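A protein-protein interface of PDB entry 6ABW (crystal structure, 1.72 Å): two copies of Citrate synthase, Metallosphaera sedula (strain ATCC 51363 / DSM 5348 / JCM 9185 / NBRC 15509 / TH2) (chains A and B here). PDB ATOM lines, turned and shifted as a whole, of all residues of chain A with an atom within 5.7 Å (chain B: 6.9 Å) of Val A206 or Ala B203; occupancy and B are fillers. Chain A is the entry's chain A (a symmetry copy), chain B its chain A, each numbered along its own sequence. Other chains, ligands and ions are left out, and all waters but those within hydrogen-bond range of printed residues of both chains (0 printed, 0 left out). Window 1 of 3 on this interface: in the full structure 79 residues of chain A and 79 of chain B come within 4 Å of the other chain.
OG of Ser A209 sits at hydrogen-bond distance from N of Ile A369, 3.3 Å away.
O of Ala A203 sits at hydrogen-bond distance from OG1 of Thr A207 (3.0 Å).
OG of Ser A209 sits at hydrogen-bond distance from O of Val A206, at 2.7 Å.
OG1 of Thr A210 lies within hydrogen-bond range of O of Thr A207 (3.0 Å).
The backbone carbonyl oxygen of Ala B203 sits at hydrogen-bond distance from the side-chain hydroxyl of Thr B207 (3.0 Å).
OG1 of Thr A210 is in hydrogen-bond range of O of Ala B224, at 2.8 Å.
Of the 20 printed residues of chain B, 5 touch a printed residue of chain A.
Hydrophobic or aromatic side chains of chain B that line the printed part of chain A: Ala B199, Val B206 and Ala B223.
Of the 12 printed residues of chain A, 5 touch a printed residue of chain B.
Hydrophobic or aromatic side chains of chain A within 4 Å of the printed part of chain B: Val A206.
Among the printed residues, no Asp or Glu carboxylate lies within 4 Å of a Lys or Arg side-chain nitrogen of the other chain.
N of Ala A203 touches CG1 of Val B206, at 3.8 Å.
Val A206 touches Ala B199 (CG1 to O, 3.6 Å).
CG1 of Val A206 touches N of Ala B203, at 3.8 Å.
Thr A207 touches Ala B223.
CG2 of Thr A207 touches N of Ala B224, at 3.9 Å.
Thr A210 touches Ala B199.
Ile A369 touches Ala B199 (O to N, 3.8 Å).
Of the printed residues of chain B, Ala A203 touches Val B206.
Of chain B, only Ala B199 (3.6 Å) and Ala B203 (3.8 Å) come within 4 Å of Val A206.
Ser A209 touches none of the printed residues of chain B.
Of the printed residues of chain B, Thr A210 touches Ala B199 (3.3 Å) and Ala B224 (2.8 Å).
Of chain A, only Val A206 comes within 4 Å of Ala B203.
Of the printed residues of chain A, Val B206 touches Ala A203.
Ala A203 touches Val B206, and with the chains exchanged Val A206 touches Ala B203.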
ATOM      1  N   THR A 201      20.676  32.289  21.716  1.00  0.00           N
ATOM      2  CA  THR A 201      19.553  31.780  22.477  1.00  0.00           C
ATOM      3  C   THR A 201      18.952  30.596  21.713  1.00  0.00           C
ATOM      4  O   THR A 201      18.642  29.571  22.328  1.00  0.00           O
ATOM      5  CB  THR A 201      18.509  32.902  22.749  1.00  0.00           C
ATOM      6  OG1 THR A 201      19.137  33.994  23.428  1.00  0.00           O
ATOM      7  CG2 THR A 201      17.394  32.403  23.632  1.00  0.00           C
ATOM      8  N   THR A 202      18.841  30.704  20.399  1.00  0.00           N
ATOM      9  CA  THR A 202      18.322  29.610  19.575  1.00  0.00           C
ATOM     10  C   THR A 202      19.176  28.315  19.734  1.00  0.00           C
ATOM     11  O   THR A 202      18.617  27.254  19.932  1.00  0.00           O
ATOM     12  CB  THR A 202      18.201  30.027  18.118  1.00  0.00           C
ATOM     13  OG1 THR A 202      17.390  31.196  17.996  1.00  0.00           O
ATOM     14  CG2 THR A 202      17.628  28.926  17.270  1.00  0.00           C
ATOM     15  N   ALA A 203      20.518  28.448  19.713  1.00  0.00           N
ATOM     16  CA  ALA A 203      21.383  27.285  19.923  1.00  0.00           C
ATOM     17  C   ALA A 203      21.174  26.666  21.282  1.00  0.00           C
ATOM     18  O   ALA A 203      21.159  25.438  21.407  1.00  0.00           O
ATOM     19  CB  ALA A 203      22.834  27.645  19.726  1.00  0.00           C
ATOM     20  N   ALA A 204      21.035  27.494  22.303  1.00  0.00           N
ATOM     21  CA  ALA A 204      20.726  27.008  23.669  1.00  0.00           C
ATOM     22  C   ALA A 204      19.424  26.222  23.680  1.00  0.00           C
ATOM     23  O   ALA A 204      19.414  25.172  24.246  1.00  0.00           O
ATOM     24  CB  ALA A 204      20.706  28.108  24.673  1.00  0.00           C
ATOM     25  N   LEU A 205      18.380  26.726  23.021  1.00  0.00           N
ATOM     26  CA  LEU A 205      17.109  26.090  22.975  1.00  0.00           C
ATOM     27  C   LEU A 205      17.155  24.735  22.260  1.00  0.00           C
ATOM     28  O   LEU A 205      16.650  23.747  22.762  1.00  0.00           O
ATOM     29  CB  LEU A 205      16.077  27.022  22.356  1.00  0.00           C
ATOM     30  CG  LEU A 205      15.743  28.270  23.176  1.00  0.00           C
ATOM     31  CD1 LEU A 205      14.868  29.214  22.319  1.00  0.00           C
ATOM     32  CD2 LEU A 205      14.973  27.931  24.456  1.00  0.00           C
ATOM     33  N   VAL A 206      17.847  24.673  21.132  1.00  0.00           N
ATOM     34  CA  VAL A 206      18.032  23.424  20.412  1.00  0.00           C
ATOM     35  C   VAL A 206      18.739  22.376  21.274  1.00  0.00           C
ATOM     36  O   VAL A 206      18.369  21.213  21.323  1.00  0.00           O
ATOM     37  CB  VAL A 206      18.876  23.633  19.138  1.00  0.00           C
ATOM     38  CG1 VAL A 206      19.170  22.290  18.460  1.00  0.00           C
ATOM     39  CG2 VAL A 206      18.075  24.461  18.185  1.00  0.00           C
ATOM     40  N   THR A 207      19.756  22.797  21.979  1.00  0.00           N
ATOM     41  CA  THR A 207      20.510  21.933  22.822  1.00  0.00           C
ATOM     42  C   THR A 207      19.616  21.448  23.977  1.00  0.00           C
ATOM     43  O   THR A 207      19.665  20.263  24.362  1.00  0.00           O
ATOM     44  CB  THR A 207      21.789  22.659  23.303  1.00  0.00           C
ATOM     45  OG1 THR A 207      22.598  22.956  22.138  1.00  0.00           O
ATOM     46  CG2 THR A 207      22.612  21.797  24.172  1.00  0.00           C
ATOM     47  N   SER A 208      18.783  22.338  24.534  1.00  0.00           N
ATOM     48  CA  SER A 208      17.940  21.982  25.658  1.00  0.00           C
ATOM     49  C   SER A 208      16.882  20.940  25.233  1.00  0.00           C
ATOM     50  O   SER A 208      16.409  20.151  26.074  1.00  0.00           O
ATOM     51  CB  SER A 208      17.269  23.214  26.276  1.00  0.00           C
ATOM     52  OG  SER A 208      16.190  23.676  25.471  1.00  0.00           O
ATOM     53  N   SER A 209      16.539  20.924  23.962  1.00  0.00           N
ATOM     54  CA  SER A 209      15.510  19.973  23.432  1.00  0.00           C
ATOM     55  C   SER A 209      15.885  18.496  23.549  1.00  0.00           C
ATOM     56  O   SER A 209      15.020  17.608  23.461  1.00  0.00           O
ATOM     57  CB  SER A 209      15.149  20.293  21.966  1.00  0.00           C
ATOM     58  OG  SER A 209      16.094  19.826  20.982  1.00  0.00           O
ATOM     59  N   THR A 210      17.154  18.212  23.666  1.00  0.00           N
ATOM     60  CA  THR A 210      17.611  16.851  23.879  1.00  0.00           C
ATOM     61  C   THR A 210      17.812  16.541  25.353  1.00  0.00           C
ATOM     62  O   THR A 210      18.293  15.465  25.682  1.00  0.00           O
ATOM     63  CB  THR A 210      18.951  16.600  23.151  1.00  0.00           C
ATOM     64  OG1 THR A 210      19.991  17.321  23.824  1.00  0.00           O
ATOM     65  CG2 THR A 210      18.906  17.029  21.699  1.00  0.00           C
ATOM     66  N   ALA A 220      26.645  25.832  23.726  1.00  0.00           N
ATOM     67  CA  ALA A 220      26.128  26.037  22.385  1.00  0.00           C
ATOM     68  C   ALA A 220      25.844  27.540  22.068  1.00  0.00           C
ATOM     69  O   ALA A 220      26.109  28.042  20.962  1.00  0.00           O
ATOM     70  CB  ALA A 220      24.873  25.233  22.190  1.00  0.00           C
ATOM     71  N   ILE A 369      13.585  18.810  19.065  1.00  0.00           N
ATOM     72  CA  ILE A 369      13.737  19.544  17.789  1.00  0.00           C
ATOM     73  C   ILE A 369      14.218  18.550  16.671  1.00  0.00           C
ATOM     74  O   ILE A 369      15.292  17.907  16.781  1.00  0.00           O
ATOM     75  CB  ILE A 369      14.530  20.899  17.953  1.00  0.00           C
ATOM     76  CG1 ILE A 369      13.627  21.943  18.660  1.00  0.00           C
ATOM     77  CG2 ILE A 369      14.987  21.432  16.602  1.00  0.00           C
ATOM     78  CD1 ILE A 369      14.290  23.193  19.221  1.00  0.00           C
ATOM     79  N   PRO B 198      18.910  15.527  12.841  1.00  0.00           N
ATOM     80  CA  PRO B 198      18.632  15.472  14.286  1.00  0.00           C
ATOM     81  C   PRO B 198      19.153  16.728  14.992  1.00  0.00           C
ATOM     82  O   PRO B 198      19.677  17.617  14.329  1.00  0.00           O
ATOM     83  CB  PRO B 198      19.341  14.209  14.741  1.00  0.00           C
ATOM     84  CG  PRO B 198      20.519  14.138  13.830  1.00  0.00           C
ATOM     85  CD  PRO B 198      20.022  14.632  12.466  1.00  0.00           C
ATOM     86  N   ALA B 199      18.920  16.833  16.289  1.00  0.00           N
ATOM     87  CA  ALA B 199      19.206  18.061  17.038  1.00  0.00           C
ATOM     88  C   ALA B 199      20.651  18.465  16.913  1.00  0.00           C
ATOM     89  O   ALA B 199      20.959  19.636  16.903  1.00  0.00           O
ATOM     90  CB  ALA B 199      18.826  17.935  18.510  1.00  0.00           C
ATOM     91  N   SER B 200      21.556  17.491  16.906  1.00  0.00           N
ATOM     92  CA  SER B 200      22.968  17.822  16.739  1.00  0.00           C
ATOM     93  C   SER B 200      23.290  18.541  15.417  1.00  0.00           C
ATOM     94  O   SER B 200      23.950  19.574  15.404  1.00  0.00           O
ATOM     95  CB  SER B 200      23.832  16.585  16.900  1.00  0.00           C
ATOM     96  OG  SER B 200      23.429  15.516  16.014  1.00  0.00           O
ATOM     97  N   THR B 201      22.710  18.091  14.324  1.00  0.00           N
ATOM     98  CA  THR B 201      22.912  18.738  13.044  1.00  0.00           C
ATOM     99  C   THR B 201      22.239  20.113  13.089  1.00  0.00           C
ATOM    100  O   THR B 201      22.833  21.095  12.635  1.00  0.00           O
ATOM    101  CB  THR B 201      22.375  17.853  11.881  1.00  0.00           C
ATOM    102  OG1 THR B 201      23.011  16.571  11.913  1.00  0.00           O
ATOM    103  CG2 THR B 201      22.681  18.474  10.541  1.00  0.00           C
ATOM    104  N   THR B 202      21.055  20.200  13.673  1.00  0.00           N
ATOM    105  CA  THR B 202      20.351  21.477  13.808  1.00  0.00           C
ATOM    106  C   THR B 202      21.196  22.517  14.606  1.00  0.00           C
ATOM    107  O   THR B 202      21.325  23.643  14.167  1.00  0.00           O
ATOM    108  CB  THR B 202      18.973  21.286  14.420  1.00  0.00           C
ATOM    109  OG1 THR B 202      18.209  20.354  13.653  1.00  0.00           O
ATOM    110  CG2 THR B 202      18.224  22.586  14.523  1.00  0.00           C
ATOM    111  N   ALA B 203      21.809  22.091  15.730  1.00  0.00           N
ATOM    112  CA  ALA B 203      22.671  22.994  16.494  1.00  0.00           C
ATOM    113  C   ALA B 203      23.851  23.467  15.681  1.00  0.00           C
ATOM    114  O   ALA B 203      24.224  24.641  15.759  1.00  0.00           O
ATOM    115  CB  ALA B 203      23.139  22.346  17.773  1.00  0.00           C
ATOM    116  N   ALA B 204      24.455  22.569  14.924  1.00  0.00           N
ATOM    117  CA  ALA B 204      25.562  22.936  14.008  1.00  0.00           C
ATOM    118  C   ALA B 204      25.107  23.986  13.005  1.00  0.00           C
ATOM    119  O   ALA B 204      25.814  24.931  12.832  1.00  0.00           O
ATOM    120  CB  ALA B 204      26.150  21.750  13.323  1.00  0.00           C
ATOM    121  N   LEU B 205      23.925  23.816  12.409  1.00  0.00           N
ATOM    122  CA  LEU B 205      23.404  24.721  11.446  1.00  0.00           C
ATOM    123  C   LEU B 205      23.129  26.111  12.031  1.00  0.00           C
ATOM    124  O   LEU B 205      23.524  27.115  11.468  1.00  0.00           O
ATOM    125  CB  LEU B 205      22.166  24.130  10.784  1.00  0.00           C
ATOM    126  CG  LEU B 205      22.413  22.895   9.914  1.00  0.00           C
ATOM    127  CD1 LEU B 205      21.049  22.287   9.509  1.00  0.00           C
ATOM    128  CD2 LEU B 205      23.186  23.234   8.637  1.00  0.00           C
ATOM    129  N   VAL B 206      22.534  26.158  13.215  1.00  0.00           N
ATOM    130  CA  VAL B 206      22.300  27.414  13.906  1.00  0.00           C
ATOM    131  C   VAL B 206      23.608  28.160  14.179  1.00  0.00           C
ATOM    132  O   VAL B 206      23.728  29.360  13.990  1.00  0.00           O
ATOM    133  CB  VAL B 206      21.597  27.184  15.260  1.00  0.00           C
ATOM    134  CG1 VAL B 206      21.473  28.501  16.032  1.00  0.00           C
ATOM    135  CG2 VAL B 206      20.215  26.684  14.982  1.00  0.00           C
ATOM    136  N   THR B 207      24.606  27.436  14.612  1.00  0.00           N
ATOM    137  CA  THR B 207      25.881  27.995  14.911  1.00  0.00           C
ATOM    138  C   THR B 207      26.522  28.518  13.614  1.00  0.00           C
ATOM    139  O   THR B 207      27.135  29.604  13.603  1.00  0.00           O
ATOM    140  CB  THR B 207      26.752  26.946  15.643  1.00  0.00           C
ATOM    141  OG1 THR B 207      26.104  26.624  16.898  1.00  0.00           O
ATOM    142  CG2 THR B 207      28.081  27.485  15.988  1.00  0.00           C
ATOM    143  N   SER B 208      26.381  27.775  12.508  1.00  0.00           N
ATOM    144  CA  SER B 208      26.991  28.165  11.253  1.00  0.00           C
ATOM    145  C   SER B 208      26.346  29.463  10.719  1.00  0.00           C
ATOM    146  O   SER B 208      26.998  30.225   9.977  1.00  0.00           O
ATOM    147  CB  SER B 208      26.904  27.047  10.209  1.00  0.00           C
ATOM    148  OG  SER B 208      25.593  26.944   9.665  1.00  0.00           O
ATOM    149  N   SER B 216      33.525  25.126  16.072  1.00  0.00           N
ATOM    150  CA  SER B 216      32.477  25.565  16.995  1.00  0.00           C
ATOM    151  C   SER B 216      31.112  25.027  16.553  1.00  0.00           C
ATOM    152  O   SER B 216      30.301  24.755  17.419  1.00  0.00           O
ATOM    153  CB  SER B 216      32.440  27.077  17.196  1.00  0.00           C
ATOM    154  OG  SER B 216      33.401  27.374  18.212  1.00  0.00           O
ATOM    155  N   CYS B 217      30.901  24.861  15.245  1.00  0.00           N
ATOM    156  CA  CYS B 217      29.715  24.153  14.769  1.00  0.00           C
ATOM    157  C   CYS B 217      29.662  22.726  15.329  1.00  0.00           C
ATOM    158  O   CYS B 217      28.618  22.306  15.826  1.00  0.00           O
ATOM    159  CB  CYS B 217      29.609  24.192  13.244  1.00  0.00           C
ATOM    160  SG  CYS B 217      29.487  25.872  12.591  1.00  0.00           S
ATOM    161  N   VAL B 219      31.237  21.735  18.105  1.00  0.00           N
ATOM    162  CA  VAL B 219      31.022  21.902  19.555  1.00  0.00           C
ATOM    163  C   VAL B 219      29.521  21.942  19.867  1.00  0.00           C
ATOM    164  O   VAL B 219      29.048  21.224  20.779  1.00  0.00           O
ATOM    165  CB  VAL B 219      31.718  23.154  20.123  1.00  0.00           C
ATOM    166  CG1 VAL B 219      31.314  23.481  21.537  1.00  0.00           C
ATOM    167  CG2 VAL B 219      33.171  22.939  20.034  1.00  0.00           C
ATOM    168  N   ALA B 220      28.785  22.738  19.105  1.00  0.00           N
ATOM    169  CA  ALA B 220      27.357  22.825  19.349  1.00  0.00           C
ATOM    170  C   ALA B 220      26.613  21.476  19.087  1.00  0.00           C
ATOM    171  O   ALA B 220      25.702  21.071  19.827  1.00  0.00           O
ATOM    172  CB  ALA B 220      26.756  23.907  18.497  1.00  0.00           C
ATOM    173  N   ALA B 221      27.014  20.805  18.030  1.00  0.00           N
ATOM    174  CA  ALA B 221      26.505  19.482  17.747  1.00  0.00           C
ATOM    175  C   ALA B 221      26.719  18.513  18.859  1.00  0.00           C
ATOM    176  O   ALA B 221      25.777  17.795  19.287  1.00  0.00           O
ATOM    177  CB  ALA B 221      27.053  18.958  16.419  1.00  0.00           C
ATOM    178  N   LEU B 222      27.941  18.509  19.405  1.00  0.00           N
ATOM    179  CA  LEU B 222      28.232  17.671  20.539  1.00  0.00           C
ATOM    180  C   LEU B 222      27.531  18.010  21.829  1.00  0.00           C
ATOM    181  O   LEU B 222      27.135  17.117  22.574  1.00  0.00           O
ATOM    182  CB  LEU B 222      29.732  17.648  20.777  1.00  0.00           C
ATOM    183  CG  LEU B 222      30.598  17.008  19.664  1.00  0.00           C
ATOM    184  CD1 LEU B 222      32.020  17.469  19.895  1.00  0.00           C
ATOM    185  CD2 LEU B 222      30.539  15.484  19.640  1.00  0.00           C
ATOM    186  N   ALA B 223      27.329  19.306  22.061  1.00  0.00           N
ATOM    187  CA  ALA B 223      26.505  19.780  23.176  1.00  0.00           C
ATOM    188  C   ALA B 223      25.095  19.201  23.103  1.00  0.00           C
ATOM    189  O   ALA B 223      24.552  18.729  24.099  1.00  0.00           O
ATOM    190  CB  ALA B 223      26.421  21.318  23.207  1.00  0.00           C
ATOM    191  N   ALA B 224      24.493  19.212  21.931  1.00  0.00           N
ATOM    192  CA  ALA B 224      23.185  18.607  21.754  1.00  0.00           C
ATOM    193  C   ALA B 224      23.181  17.063  21.845  1.00  0.00           C
ATOM    194  O   ALA B 224      22.299  16.458  22.487  1.00  0.00           O
ATOM    195  CB  ALA B 224      22.606  19.032  20.400  1.00  0.00           C
ATOM    196  N   VAL B 358      26.928  21.855   7.238  1.00  0.00           N
ATOM    197  CA  VAL B 358      27.145  23.244   7.513  1.00  0.00           C
ATOM    198  C   VAL B 358      27.797  23.923   6.293  1.00  0.00           C
ATOM    199  O   VAL B 358      27.416  25.051   5.994  1.00  0.00           O
ATOM    200  CB  VAL B 358      27.891  23.585   8.815  1.00  0.00           C
ATOM    201  CG1 VAL B 358      27.029  23.106   9.999  1.00  0.00           C
ATOM    202  CG2 VAL B 358      29.274  23.018   8.898  1.00  0.00           C
